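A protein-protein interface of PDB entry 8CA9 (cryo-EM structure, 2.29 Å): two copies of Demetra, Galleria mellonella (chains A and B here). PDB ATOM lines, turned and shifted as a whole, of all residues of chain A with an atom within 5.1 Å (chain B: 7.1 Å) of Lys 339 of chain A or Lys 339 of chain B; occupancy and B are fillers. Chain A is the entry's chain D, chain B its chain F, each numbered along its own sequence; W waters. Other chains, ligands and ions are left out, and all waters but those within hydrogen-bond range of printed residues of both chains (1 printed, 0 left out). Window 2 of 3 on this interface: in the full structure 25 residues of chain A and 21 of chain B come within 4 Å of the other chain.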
ATOM      1  N   ASP A 335      -9.363  -7.273   8.542  1.00  0.00           N
ATOM      2  CA  ASP A 335      -8.415  -6.173   8.660  1.00  0.00           C
ATOM      3  C   ASP A 335      -6.991  -6.706   8.681  1.00  0.00           C
ATOM      4  O   ASP A 335      -6.148  -6.296   7.872  1.00  0.00           O
ATOM      5  CB  ASP A 335      -8.713  -5.356   9.917  1.00  0.00           C
ATOM      6  CG  ASP A 335      -8.373  -3.889   9.751  1.00  0.00           C
ATOM      7  OD1 ASP A 335      -8.862  -3.273   8.781  1.00  0.00           O
ATOM      8  OD2 ASP A 335      -7.626  -3.348  10.593  1.00  0.00           O
ATOM      9  N   SER A 336      -6.726  -7.680   9.553  1.00  0.00           N
ATOM     10  CA  SER A 336      -5.379  -8.225   9.641  1.00  0.00           C
ATOM     11  C   SER A 336      -4.928  -8.740   8.283  1.00  0.00           C
ATOM     12  O   SER A 336      -3.831  -8.415   7.814  1.00  0.00           O
ATOM     13  CB  SER A 336      -5.328  -9.337  10.688  1.00  0.00           C
ATOM     14  OG  SER A 336      -4.009  -9.835  10.836  1.00  0.00           O
ATOM     15  N   TYR A 337      -5.795  -9.501   7.610  1.00  0.00           N
ATOM     16  CA  TYR A 337      -5.400 -10.101   6.343  1.00  0.00           C
ATOM     17  C   TYR A 337      -4.963  -9.032   5.353  1.00  0.00           C
ATOM     18  O   TYR A 337      -4.064  -9.261   4.536  1.00  0.00           O
ATOM     19  CB  TYR A 337      -6.549 -10.932   5.773  1.00  0.00           C
ATOM     20  CG  TYR A 337      -6.091 -12.106   4.937  1.00  0.00           C
ATOM     21  CD1 TYR A 337      -5.676 -13.287   5.537  1.00  0.00           C
ATOM     22  CD2 TYR A 337      -6.074 -12.034   3.552  1.00  0.00           C
ATOM     23  CE1 TYR A 337      -5.256 -14.362   4.780  1.00  0.00           C
ATOM     24  CE2 TYR A 337      -5.656 -13.105   2.787  1.00  0.00           C
ATOM     25  CZ  TYR A 337      -5.247 -14.267   3.406  1.00  0.00           C
ATOM     26  OH  TYR A 337      -4.830 -15.337   2.650  1.00  0.00           O
ATOM     27  N   GLU A 338      -5.585  -7.852   5.411  1.00  0.00           N
ATOM     28  CA  GLU A 338      -5.156  -6.764   4.542  1.00  0.00           C
ATOM     29  C   GLU A 338      -3.810  -6.207   4.992  1.00  0.00           C
ATOM     30  O   GLU A 338      -2.871  -6.099   4.192  1.00  0.00           O
ATOM     31  CB  GLU A 338      -6.218  -5.666   4.517  1.00  0.00           C
ATOM     32  CG  GLU A 338      -7.544  -6.109   3.917  1.00  0.00           C
ATOM     33  CD  GLU A 338      -8.608  -5.030   3.981  1.00  0.00           C
ATOM     34  OE1 GLU A 338      -8.318  -3.935   4.505  1.00  0.00           O
ATOM     35  OE2 GLU A 338      -9.736  -5.279   3.506  1.00  0.00           O
ATOM     36  N   LYS A 339      -3.680  -5.901   6.286  1.00  0.00           N
ATOM     37  CA  LYS A 339      -2.485  -5.206   6.753  1.00  0.00           C
ATOM     38  C   LYS A 339      -1.236  -6.030   6.488  1.00  0.00           C
ATOM     39  O   LYS A 339      -0.223  -5.503   6.011  1.00  0.00           O
ATOM     40  CB  LYS A 339      -2.606  -4.884   8.243  1.00  0.00           C
ATOM     41  CG  LYS A 339      -3.748  -3.945   8.582  1.00  0.00           C
ATOM     42  CD  LYS A 339      -3.404  -3.080   9.781  1.00  0.00           C
ATOM     43  CE  LYS A 339      -4.581  -2.219  10.209  1.00  0.00           C
ATOM     44  NZ  LYS A 339      -5.266  -1.578   9.055  1.00  0.00           N
ATOM     45  N   THR A 340      -1.298  -7.334   6.764  1.00  0.00           N
ATOM     46  CA  THR A 340      -0.166  -8.206   6.483  1.00  0.00           C
ATOM     47  C   THR A 340       0.314  -8.011   5.051  1.00  0.00           C
ATOM     48  O   THR A 340       1.512  -7.832   4.802  1.00  0.00           O
ATOM     49  CB  THR A 340      -0.559  -9.663   6.732  1.00  0.00           C
ATOM     50  OG1 THR A 340      -0.835  -9.856   8.124  1.00  0.00           O
ATOM     51  CG2 THR A 340       0.553 -10.609   6.300  1.00  0.00           C
ATOM     52  N   PHE A 341      -0.619  -7.998   4.097  1.00  0.00           N
ATOM     53  CA  PHE A 341      -0.231  -7.822   2.703  1.00  0.00           C
ATOM     54  C   PHE A 341       0.540  -6.522   2.523  1.00  0.00           C
ATOM     55  O   PHE A 341       1.614  -6.501   1.911  1.00  0.00           O
ATOM     56  CB  PHE A 341      -1.466  -7.849   1.804  1.00  0.00           C
ATOM     57  CG  PHE A 341      -1.146  -7.870   0.338  1.00  0.00           C
ATOM     58  CD1 PHE A 341      -0.701  -9.031  -0.270  1.00  0.00           C
ATOM     59  CD2 PHE A 341      -1.290  -6.730  -0.434  1.00  0.00           C
ATOM     60  CE1 PHE A 341      -0.404  -9.054  -1.618  1.00  0.00           C
ATOM     61  CE2 PHE A 341      -0.995  -6.747  -1.782  1.00  0.00           C
ATOM     62  CZ  PHE A 341      -0.552  -7.911  -2.375  1.00  0.00           C
ATOM     63  N   LEU A 342       0.024  -5.428   3.090  1.00  0.00           N
ATOM     64  CA  LEU A 342       0.739  -4.161   3.006  1.00  0.00           C
ATOM     65  C   LEU A 342       2.147  -4.300   3.566  1.00  0.00           C
ATOM     66  O   LEU A 342       3.114  -3.813   2.967  1.00  0.00           O
ATOM     67  CB  LEU A 342      -0.035  -3.070   3.746  1.00  0.00           C
ATOM     68  CG  LEU A 342      -1.373  -2.666   3.119  1.00  0.00           C
ATOM     69  CD1 LEU A 342      -2.141  -1.728   4.035  1.00  0.00           C
ATOM     70  CD2 LEU A 342      -1.160  -2.021   1.757  1.00  0.00           C
ATOM     71  N   GLN A 343       2.288  -5.000   4.695  1.00  0.00           N
ATOM     72  CA  GLN A 343       3.616  -5.204   5.261  1.00  0.00           C
ATOM     73  C   GLN A 343       4.522  -5.916   4.269  1.00  0.00           C
ATOM     74  O   GLN A 343       5.688  -5.541   4.102  1.00  0.00           O
ATOM     75  CB  GLN A 343       3.514  -5.989   6.569  1.00  0.00           C
ATOM     76  CG  GLN A 343       2.801  -5.238   7.679  1.00  0.00           C
ATOM     77  CD  GLN A 343       2.702  -6.041   8.961  1.00  0.00           C
ATOM     78  OE1 GLN A 343       2.971  -7.242   8.979  1.00  0.00           O
ATOM     79  NE2 GLN A 343       2.317  -5.377  10.045  1.00  0.00           N
ATOM     80  N   PHE A 344       3.996  -6.932   3.578  1.00  0.00           N
ATOM     81  CA  PHE A 344       4.791  -7.601   2.555  1.00  0.00           C
ATOM     82  C   PHE A 344       5.291  -6.600   1.524  1.00  0.00           C
ATOM     83  O   PHE A 344       6.459  -6.644   1.119  1.00  0.00           O
ATOM     84  CB  PHE A 344       3.968  -8.701   1.876  1.00  0.00           C
ATOM     85  CG  PHE A 344       3.635  -9.867   2.772  1.00  0.00           C
ATOM     86  CD1 PHE A 344       4.410 -10.168   3.882  1.00  0.00           C
ATOM     87  CD2 PHE A 344       2.543 -10.672   2.492  1.00  0.00           C
ATOM     88  CE1 PHE A 344       4.099 -11.241   4.693  1.00  0.00           C
ATOM     89  CE2 PHE A 344       2.227 -11.746   3.300  1.00  0.00           C
ATOM     90  CZ  PHE A 344       3.006 -12.031   4.402  1.00  0.00           C
ATOM     91  N   ILE B 331      -5.758   5.836   4.374  1.00  0.00           N
ATOM     92  CA  ILE B 331      -5.978   5.569   5.793  1.00  0.00           C
ATOM     93  C   ILE B 331      -5.334   4.246   6.170  1.00  0.00           C
ATOM     94  O   ILE B 331      -4.489   4.177   7.073  1.00  0.00           O
ATOM     95  CB  ILE B 331      -7.483   5.574   6.116  1.00  0.00           C
ATOM     96  CG1 ILE B 331      -8.068   6.982   5.970  1.00  0.00           C
ATOM     97  CG2 ILE B 331      -7.730   5.029   7.515  1.00  0.00           C
ATOM     98  CD1 ILE B 331      -7.629   7.957   7.046  1.00  0.00           C
ATOM     99  N   GLN B 332      -5.673   3.186   5.432  1.00  0.00           N
ATOM    100  CA  GLN B 332      -5.143   1.868   5.753  1.00  0.00           C
ATOM    101  C   GLN B 332      -3.630   1.931   5.882  1.00  0.00           C
ATOM    102  O   GLN B 332      -3.065   1.564   6.921  1.00  0.00           O
ATOM    103  CB  GLN B 332      -5.551   0.865   4.674  1.00  0.00           C
ATOM    104  CG  GLN B 332      -5.884  -0.522   5.196  1.00  0.00           C
ATOM    105  CD  GLN B 332      -7.256  -0.589   5.837  1.00  0.00           C
ATOM    106  OE1 GLN B 332      -7.959   0.417   5.934  1.00  0.00           O
ATOM    107  NE2 GLN B 332      -7.646  -1.780   6.275  1.00  0.00           N
ATOM    108  N   PHE B 333      -2.964   2.483   4.865  1.00  0.00           N
ATOM    109  CA  PHE B 333      -1.510   2.555   4.897  1.00  0.00           C
ATOM    110  C   PHE B 333      -1.047   3.214   6.185  1.00  0.00           C
ATOM    111  O   PHE B 333      -0.261   2.635   6.946  1.00  0.00           O
ATOM    112  CB  PHE B 333      -0.996   3.321   3.676  1.00  0.00           C
ATOM    113  CG  PHE B 333       0.486   3.554   3.685  1.00  0.00           C
ATOM    114  CD1 PHE B 333       1.357   2.584   3.221  1.00  0.00           C
ATOM    115  CD2 PHE B 333       1.010   4.746   4.155  1.00  0.00           C
ATOM    116  CE1 PHE B 333       2.722   2.798   3.229  1.00  0.00           C
ATOM    117  CE2 PHE B 333       2.371   4.965   4.164  1.00  0.00           C
ATOM    118  CZ  PHE B 333       3.228   3.991   3.700  1.00  0.00           C
ATOM    119  N   VAL B 334      -1.588   4.399   6.481  1.00  0.00           N
ATOM    120  CA  VAL B 334      -1.195   5.103   7.696  1.00  0.00           C
ATOM    121  C   VAL B 334      -1.280   4.159   8.883  1.00  0.00           C
ATOM    122  O   VAL B 334      -0.291   3.925   9.590  1.00  0.00           O
ATOM    123  CB  VAL B 334      -2.069   6.355   7.898  1.00  0.00           C
ATOM    124  CG1 VAL B 334      -1.990   6.844   9.335  1.00  0.00           C
ATOM    125  CG2 VAL B 334      -1.646   7.457   6.937  1.00  0.00           C
ATOM    126  N   ASP B 335      -2.446   3.534   9.068  1.00  0.00           N
ATOM    127  CA  ASP B 335      -2.622   2.653  10.214  1.00  0.00           C
ATOM    128  C   ASP B 335      -1.532   1.594  10.236  1.00  0.00           C
ATOM    129  O   ASP B 335      -0.816   1.438  11.234  1.00  0.00           O
ATOM    130  CB  ASP B 335      -4.009   2.011  10.174  1.00  0.00           C
ATOM    131  CG  ASP B 335      -4.569   1.750  11.558  1.00  0.00           C
ATOM    132  OD1 ASP B 335      -4.620   2.698  12.367  1.00  0.00           O
ATOM    133  OD2 ASP B 335      -4.965   0.598  11.834  1.00  0.00           O
ATOM    134  N   SER B 336      -1.340   0.904   9.109  1.00  0.00           N
ATOM    135  CA  SER B 336      -0.326  -0.139   9.064  1.00  0.00           C
ATOM    136  C   SER B 336       1.031   0.428   9.447  1.00  0.00           C
ATOM    137  O   SER B 336       1.736  -0.133  10.296  1.00  0.00           O
ATOM    138  CB  SER B 336      -0.279  -0.766   7.670  1.00  0.00           C
ATOM    139  OG  SER B 336       0.656  -1.830   7.625  1.00  0.00           O
ATOM    140  N   TYR B 337       1.389   1.578   8.872  1.00  0.00           N
ATOM    141  CA  TYR B 337       2.710   2.137   9.124  1.00  0.00           C
ATOM    142  C   TYR B 337       2.926   2.357  10.614  1.00  0.00           C
ATOM    143  O   TYR B 337       4.046   2.213  11.115  1.00  0.00           O
ATOM    144  CB  TYR B 337       2.887   3.441   8.349  1.00  0.00           C
ATOM    145  CG  TYR B 337       4.319   3.717   7.948  1.00  0.00           C
ATOM    146  CD1 TYR B 337       4.877   3.103   6.834  1.00  0.00           C
ATOM    147  CD2 TYR B 337       5.113   4.587   8.681  1.00  0.00           C
ATOM    148  CE1 TYR B 337       6.183   3.349   6.463  1.00  0.00           C
ATOM    149  CE2 TYR B 337       6.421   4.840   8.316  1.00  0.00           C
ATOM    150  CZ  TYR B 337       6.950   4.218   7.206  1.00  0.00           C
ATOM    151  OH  TYR B 337       8.253   4.466   6.838  1.00  0.00           O
ATOM    152  N   GLU B 338       1.862   2.706  11.341  1.00  0.00           N
ATOM    153  CA  GLU B 338       1.991   2.855  12.785  1.00  0.00           C
ATOM    154  C   GLU B 338       2.153   1.498  13.459  1.00  0.00           C
ATOM    155  O   GLU B 338       3.090   1.287  14.239  1.00  0.00           O
ATOM    156  CB  GLU B 338       0.777   3.599  13.344  1.00  0.00           C
ATOM    157  CG  GLU B 338       0.651   5.029  12.840  1.00  0.00           C
ATOM    158  CD  GLU B 338      -0.603   5.719  13.340  1.00  0.00           C
ATOM    159  OE1 GLU B 338      -1.387   5.078  14.071  1.00  0.00           O
ATOM    160  OE2 GLU B 338      -0.806   6.902  12.999  1.00  0.00           O
ATOM    161  N   LYS B 339       1.277   0.544  13.126  1.00  0.00           N
ATOM    162  CA  LYS B 339       1.263  -0.720  13.856  1.00  0.00           C
ATOM    163  C   LYS B 339       2.596  -1.441  13.721  1.00  0.00           C
ATOM    164  O   LYS B 339       3.141  -1.947  14.710  1.00  0.00           O
ATOM    165  CB  LYS B 339       0.125  -1.608  13.358  1.00  0.00           C
ATOM    166  CG  LYS B 339      -1.257  -1.026  13.586  1.00  0.00           C
ATOM    167  CD  LYS B 339      -2.281  -2.123  13.821  1.00  0.00           C
ATOM    168  CE  LYS B 339      -3.689  -1.565  13.931  1.00  0.00           C
ATOM    169  NZ  LYS B 339      -3.754  -0.349  14.785  1.00  0.00           N
ATOM    170  N   THR B 340       3.149  -1.472  12.507  1.00  0.00           N
ATOM    171  CA  THR B 340       4.453  -2.089  12.305  1.00  0.00           C
ATOM    172  C   THR B 340       5.461  -1.551  13.310  1.00  0.00           C
ATOM    173  O   THR B 340       6.174  -2.319  13.967  1.00  0.00           O
ATOM    174  CB  THR B 340       4.928  -1.840  10.871  1.00  0.00           C
ATOM    175  OG1 THR B 340       4.056  -2.510   9.952  1.00  0.00           O
ATOM    176  CG2 THR B 340       6.351  -2.340  10.674  1.00  0.00           C
ATOM    177  N   PHE B 341       5.501  -0.226  13.477  1.00  0.00           N
ATOM    178  CA  PHE B 341       6.446   0.358  14.421  1.00  0.00           C
ATOM    179  C   PHE B 341       6.232  -0.212  15.815  1.00  0.00           C
ATOM    180  O   PHE B 341       7.184  -0.641  16.478  1.00  0.00           O
ATOM    181  CB  PHE B 341       6.308   1.880  14.429  1.00  0.00           C
ATOM    182  CG  PHE B 341       7.371   2.578  15.225  1.00  0.00           C
ATOM    183  CD1 PHE B 341       8.652   2.716  14.719  1.00  0.00           C
ATOM    184  CD2 PHE B 341       7.091   3.097  16.477  1.00  0.00           C
ATOM    185  CE1 PHE B 341       9.635   3.357  15.449  1.00  0.00           C
ATOM    186  CE2 PHE B 341       8.069   3.740  17.210  1.00  0.00           C
ATOM    187  CZ  PHE B 341       9.342   3.870  16.694  1.00  0.00           C
ATOM    188  N   LEU B 342       4.975  -0.266  16.262  1.00  0.00           N
ATOM    189  CA  LEU B 342       4.692  -0.852  17.566  1.00  0.00           C
ATOM    190  C   LEU B 342       5.224  -2.275  17.641  1.00  0.00           C
ATOM    191  O   LEU B 342       5.840  -2.665  18.641  1.00  0.00           O
ATOM    192  CB  LEU B 342       3.188  -0.818  17.843  1.00  0.00           C
ATOM    193  CG  LEU B 342       2.582   0.575  18.037  1.00  0.00           C
ATOM    194  CD1 LEU B 342       1.066   0.501  18.106  1.00  0.00           C
ATOM    195  CD2 LEU B 342       3.140   1.238  19.289  1.00  0.00           C
ATOM    196  N   GLN B 343       5.036  -3.055  16.573  1.00  0.00           N
ATOM    197  CA  GLN B 343       5.556  -4.416  16.567  1.00  0.00           C
ATOM    198  C   GLN B 343       7.065  -4.417  16.763  1.00  0.00           C
ATOM    199  O   GLN B 343       7.598  -5.228  17.530  1.00  0.00           O
ATOM    200  CB  GLN B 343       5.175  -5.120  15.265  1.00  0.00           C
ATOM    201  CG  GLN B 343       3.681  -5.345  15.106  1.00  0.00           C
ATOM    202  CD  GLN B 343       3.326  -6.032  13.803  1.00  0.00           C
ATOM    203  OE1 GLN B 343       4.161  -6.159  12.906  1.00  0.00           O
ATOM    204  NE2 GLN B 343       2.084  -6.484  13.694  1.00  0.00           N
ATOM    205  N   PHE B 344       7.770  -3.496  16.099  1.00  0.00           N
ATOM    206  CA  PHE B 344       9.209  -3.394  16.309  1.00  0.00           C
ATOM    207  C   PHE B 344       9.524  -3.190  17.783  1.00  0.00           C
ATOM    208  O   PHE B 344      10.443  -3.818  18.325  1.00  0.00           O
ATOM    209  CB  PHE B 344       9.790  -2.249  15.475  1.00  0.00           C
ATOM    210  CG  PHE B 344       9.745  -2.482  13.985  1.00  0.00           C
ATOM    211  CD1 PHE B 344       9.690  -3.763  13.459  1.00  0.00           C
ATOM    212  CD2 PHE B 344       9.766  -1.408  13.111  1.00  0.00           C
ATOM    213  CE1 PHE B 344       9.652  -3.965  12.093  1.00  0.00           C
ATOM    214  CE2 PHE B 344       9.730  -1.606  11.745  1.00  0.00           C
ATOM    215  CZ  PHE B 344       9.672  -2.886  11.236  1.00  0.00           C
ATOM    216  N   LEU B 345       8.753  -2.334  18.459  1.00  0.00           N
ATOM    217  CA  LEU B 345       9.007  -2.080  19.872  1.00  0.00           C
ATOM    218  C   LEU B 345       8.899  -3.363  20.685  1.00  0.00           C
ATOM    219  O   LEU B 345       9.595  -3.528  21.693  1.00  0.00           O
ATOM    220  CB  LEU B 345       8.036  -1.023  20.398  1.00  0.00           C
ATOM    221  CG  LEU B 345       8.085   0.339  19.699  1.00  0.00           C
ATOM    222  CD1 LEU B 345       7.079   1.294  20.319  1.00  0.00           C
ATOM    223  CD2 LEU B 345       9.484   0.932  19.749  1.00  0.00           C
ATOM    224  N   TYR B 371      12.823   6.090   9.506  1.00  0.00           N
ATOM    225  CA  TYR B 371      11.586   5.334   9.357  1.00  0.00           C
ATOM    226  C   TYR B 371      10.378   6.257   9.359  1.00  0.00           C
ATOM    227  O   TYR B 371       9.403   6.019   8.637  1.00  0.00           O
ATOM    228  CB  TYR B 371      11.463   4.294  10.471  1.00  0.00           C
ATOM    229  CG  TYR B 371      10.187   3.488  10.392  1.00  0.00           C
ATOM    230  CD1 TYR B 371      10.101   2.367   9.580  1.00  0.00           C
ATOM    231  CD2 TYR B 371       9.066   3.852  11.125  1.00  0.00           C
ATOM    232  CE1 TYR B 371       8.936   1.629   9.502  1.00  0.00           C
ATOM    233  CE2 TYR B 371       7.898   3.122  11.054  1.00  0.00           C
ATOM    234  CZ  TYR B 371       7.838   2.011  10.241  1.00  0.00           C
ATOM    235  OH  TYR B 371       6.676   1.280  10.166  1.00  0.00           O
ATOM    236  N   TRP B 372      10.421   7.319  10.162  1.00  0.00           N
ATOM    237  CA  TRP B 372       9.292   8.231  10.259  1.00  0.00           C
ATOM    238  C   TRP B 372       9.337   9.348   9.227  1.00  0.00           C
ATOM    239  O   TRP B 372       8.403  10.155   9.173  1.00  0.00           O
ATOM    240  CB  TRP B 372       9.210   8.824  11.669  1.00  0.00           C
ATOM    241  CG  TRP B 372       8.583   7.881  12.651  1.00  0.00           C
ATOM    242  CD1 TRP B 372       9.195   7.261  13.699  1.00  0.00           C
ATOM    243  CD2 TRP B 372       7.220   7.437  12.661  1.00  0.00           C
ATOM    244  NE1 TRP B 372       8.296   6.464  14.367  1.00  0.00           N
ATOM    245  CE2 TRP B 372       7.077   6.555  13.749  1.00  0.00           C
ATOM    246  CE3 TRP B 372       6.106   7.703  11.858  1.00  0.00           C
ATOM    247  CZ2 TRP B 372       5.865   5.937  14.056  1.00  0.00           C
ATOM    248  CZ3 TRP B 372       4.906   7.090  12.164  1.00  0.00           C
ATOM    249  CH2 TRP B 372       4.795   6.217  13.253  1.00  0.00           C
ATOM    250  N   PHE B 438       5.302   8.644  19.348  1.00  0.00           N
ATOM    251  CA  PHE B 438       5.816   7.323  18.990  1.00  0.00           C
ATOM    252  C   PHE B 438       7.324   7.246  19.215  1.00  0.00           C
ATOM    253  O   PHE B 438       7.843   6.255  19.751  1.00  0.00           O
ATOM    254  CB  PHE B 438       5.483   6.991  17.534  1.00  0.00           C
ATOM    255  CG  PHE B 438       4.046   6.617  17.307  1.00  0.00           C
ATOM    256  CD1 PHE B 438       3.525   5.456  17.854  1.00  0.00           C
ATOM    257  CD2 PHE B 438       3.223   7.416  16.533  1.00  0.00           C
ATOM    258  CE1 PHE B 438       2.204   5.107  17.643  1.00  0.00           C
ATOM    259  CE2 PHE B 438       1.903   7.070  16.319  1.00  0.00           C
ATOM    260  CZ  PHE B 438       1.393   5.916  16.873  1.00  0.00           C
HETATM  261  O   HOH W   1      -0.568  -5.486  11.832  1.00  0.00           O
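Lys 339 of chain A touches Asp 335 of chain B, but with the chains exchanged Asp 335 of chain A does not touch Lys 339 of chain B (5.5 Å). Lys 339 of chain A touches its own counterpart, Lys 339 of chain B. Gln 343 of chain A touches Thr 340 of chain B, but with the chains exchanged Thr 340 of chain A does not touch Gln 343 of chain B (7.1 Å). Gln 343 of chain A touches its own counterpart, Gln 343 of chain B. Of the 7 pairs that touch across the chains among the printed residues, 2 have their exchanged pair printed and touching as well.
Water W1 lies within hydrogen-bond range of the side-chain amide nitrogen of Gln 343 of chain B and the side-chain amide nitrogen of Gln 343 of chain A.
NZ of Lys 339 of chain A is in salt-bridge range of OD2 of Asp 335 of chain A (3.3 Å). The side-chain amino group (NZ) of Lys 339 of chain B is in salt-bridge range of the side-chain carboxylate (OD2) of Asp 335 of chain B (3.3 Å). The backbone carbonyl oxygen (O) of Ser 336 of chain B lies within hydrogen-bond range of the side-chain hydroxyl (OG1) of Thr 340 of chain B (3.3 Å).
Lys 339 of chain A touches three residues of chain B. Of chain A, only Lys 339 (3.9 Å) comes within 4 Å of Lys 339 of chain B. Printed residues of chain A within 4 Å of Gln 343 of chain B: Gln 343 (3.5 Å). Printed residues of chain A within 4 Å of Thr 340 of chain B: Gln 343. Printed residues of chain B within 4 Å of Gln 343 of chain A: Thr 340 and Gln 343. Of the printed residues of chain B, Asp 335 of chain A touches Gln 332. Of the printed residues of chain A, Gln 332 of chain B touches Asp 335, Glu 338 and Lys 339. Thr 340 of chain A touches none of the printed residues of chain B. The nearest residue of chain B that does not touch Lys 339 of chain A is Ser 336 of chain B (4.1 Å). The nearest printed residue of chain A that does not touch Lys 339 of chain B is Gln 343 of chain A (5.4 Å).
The side-chain amide nitrogen of Gln 332 of chain B sits at hydrogen-bond distance from the side-chain carboxylate of Asp 335 of chain A (3.2 Å). The side-chain carboxylate (OE1) of Glu 338 of chain A sits at hydrogen-bond distance from the side-chain amide nitrogen (NE2) of Gln 332 of chain B (2.9 Å). The side-chain amino group (NZ) of Lys 339 of chain A is in salt-bridge range of the side-chain carboxylate (OD2) of Asp 335 of chain B. OG1 of Thr 340 of chain B lies within hydrogen-bond range of NE2 of Gln 343 of chain A (3.4 Å). The side-chain amide nitrogen (NE2) of Gln 343 of chain A is in hydrogen-bond range of the side-chain amide oxygen (OE1) of Gln 343 of chain B (3.5 Å).
Of the 10 printed residues of chain A, 4 touch a printed residue of chain B. Among the printed residues, 7 pairs touch across the chains.
Among the printed residues, pairs that only touch across the chains: Lys 339 of chain A with Gln 332 of chain B (3.7 Å) and Lys 339 of chain A with Lys 339 of chain B (3.9 Å).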
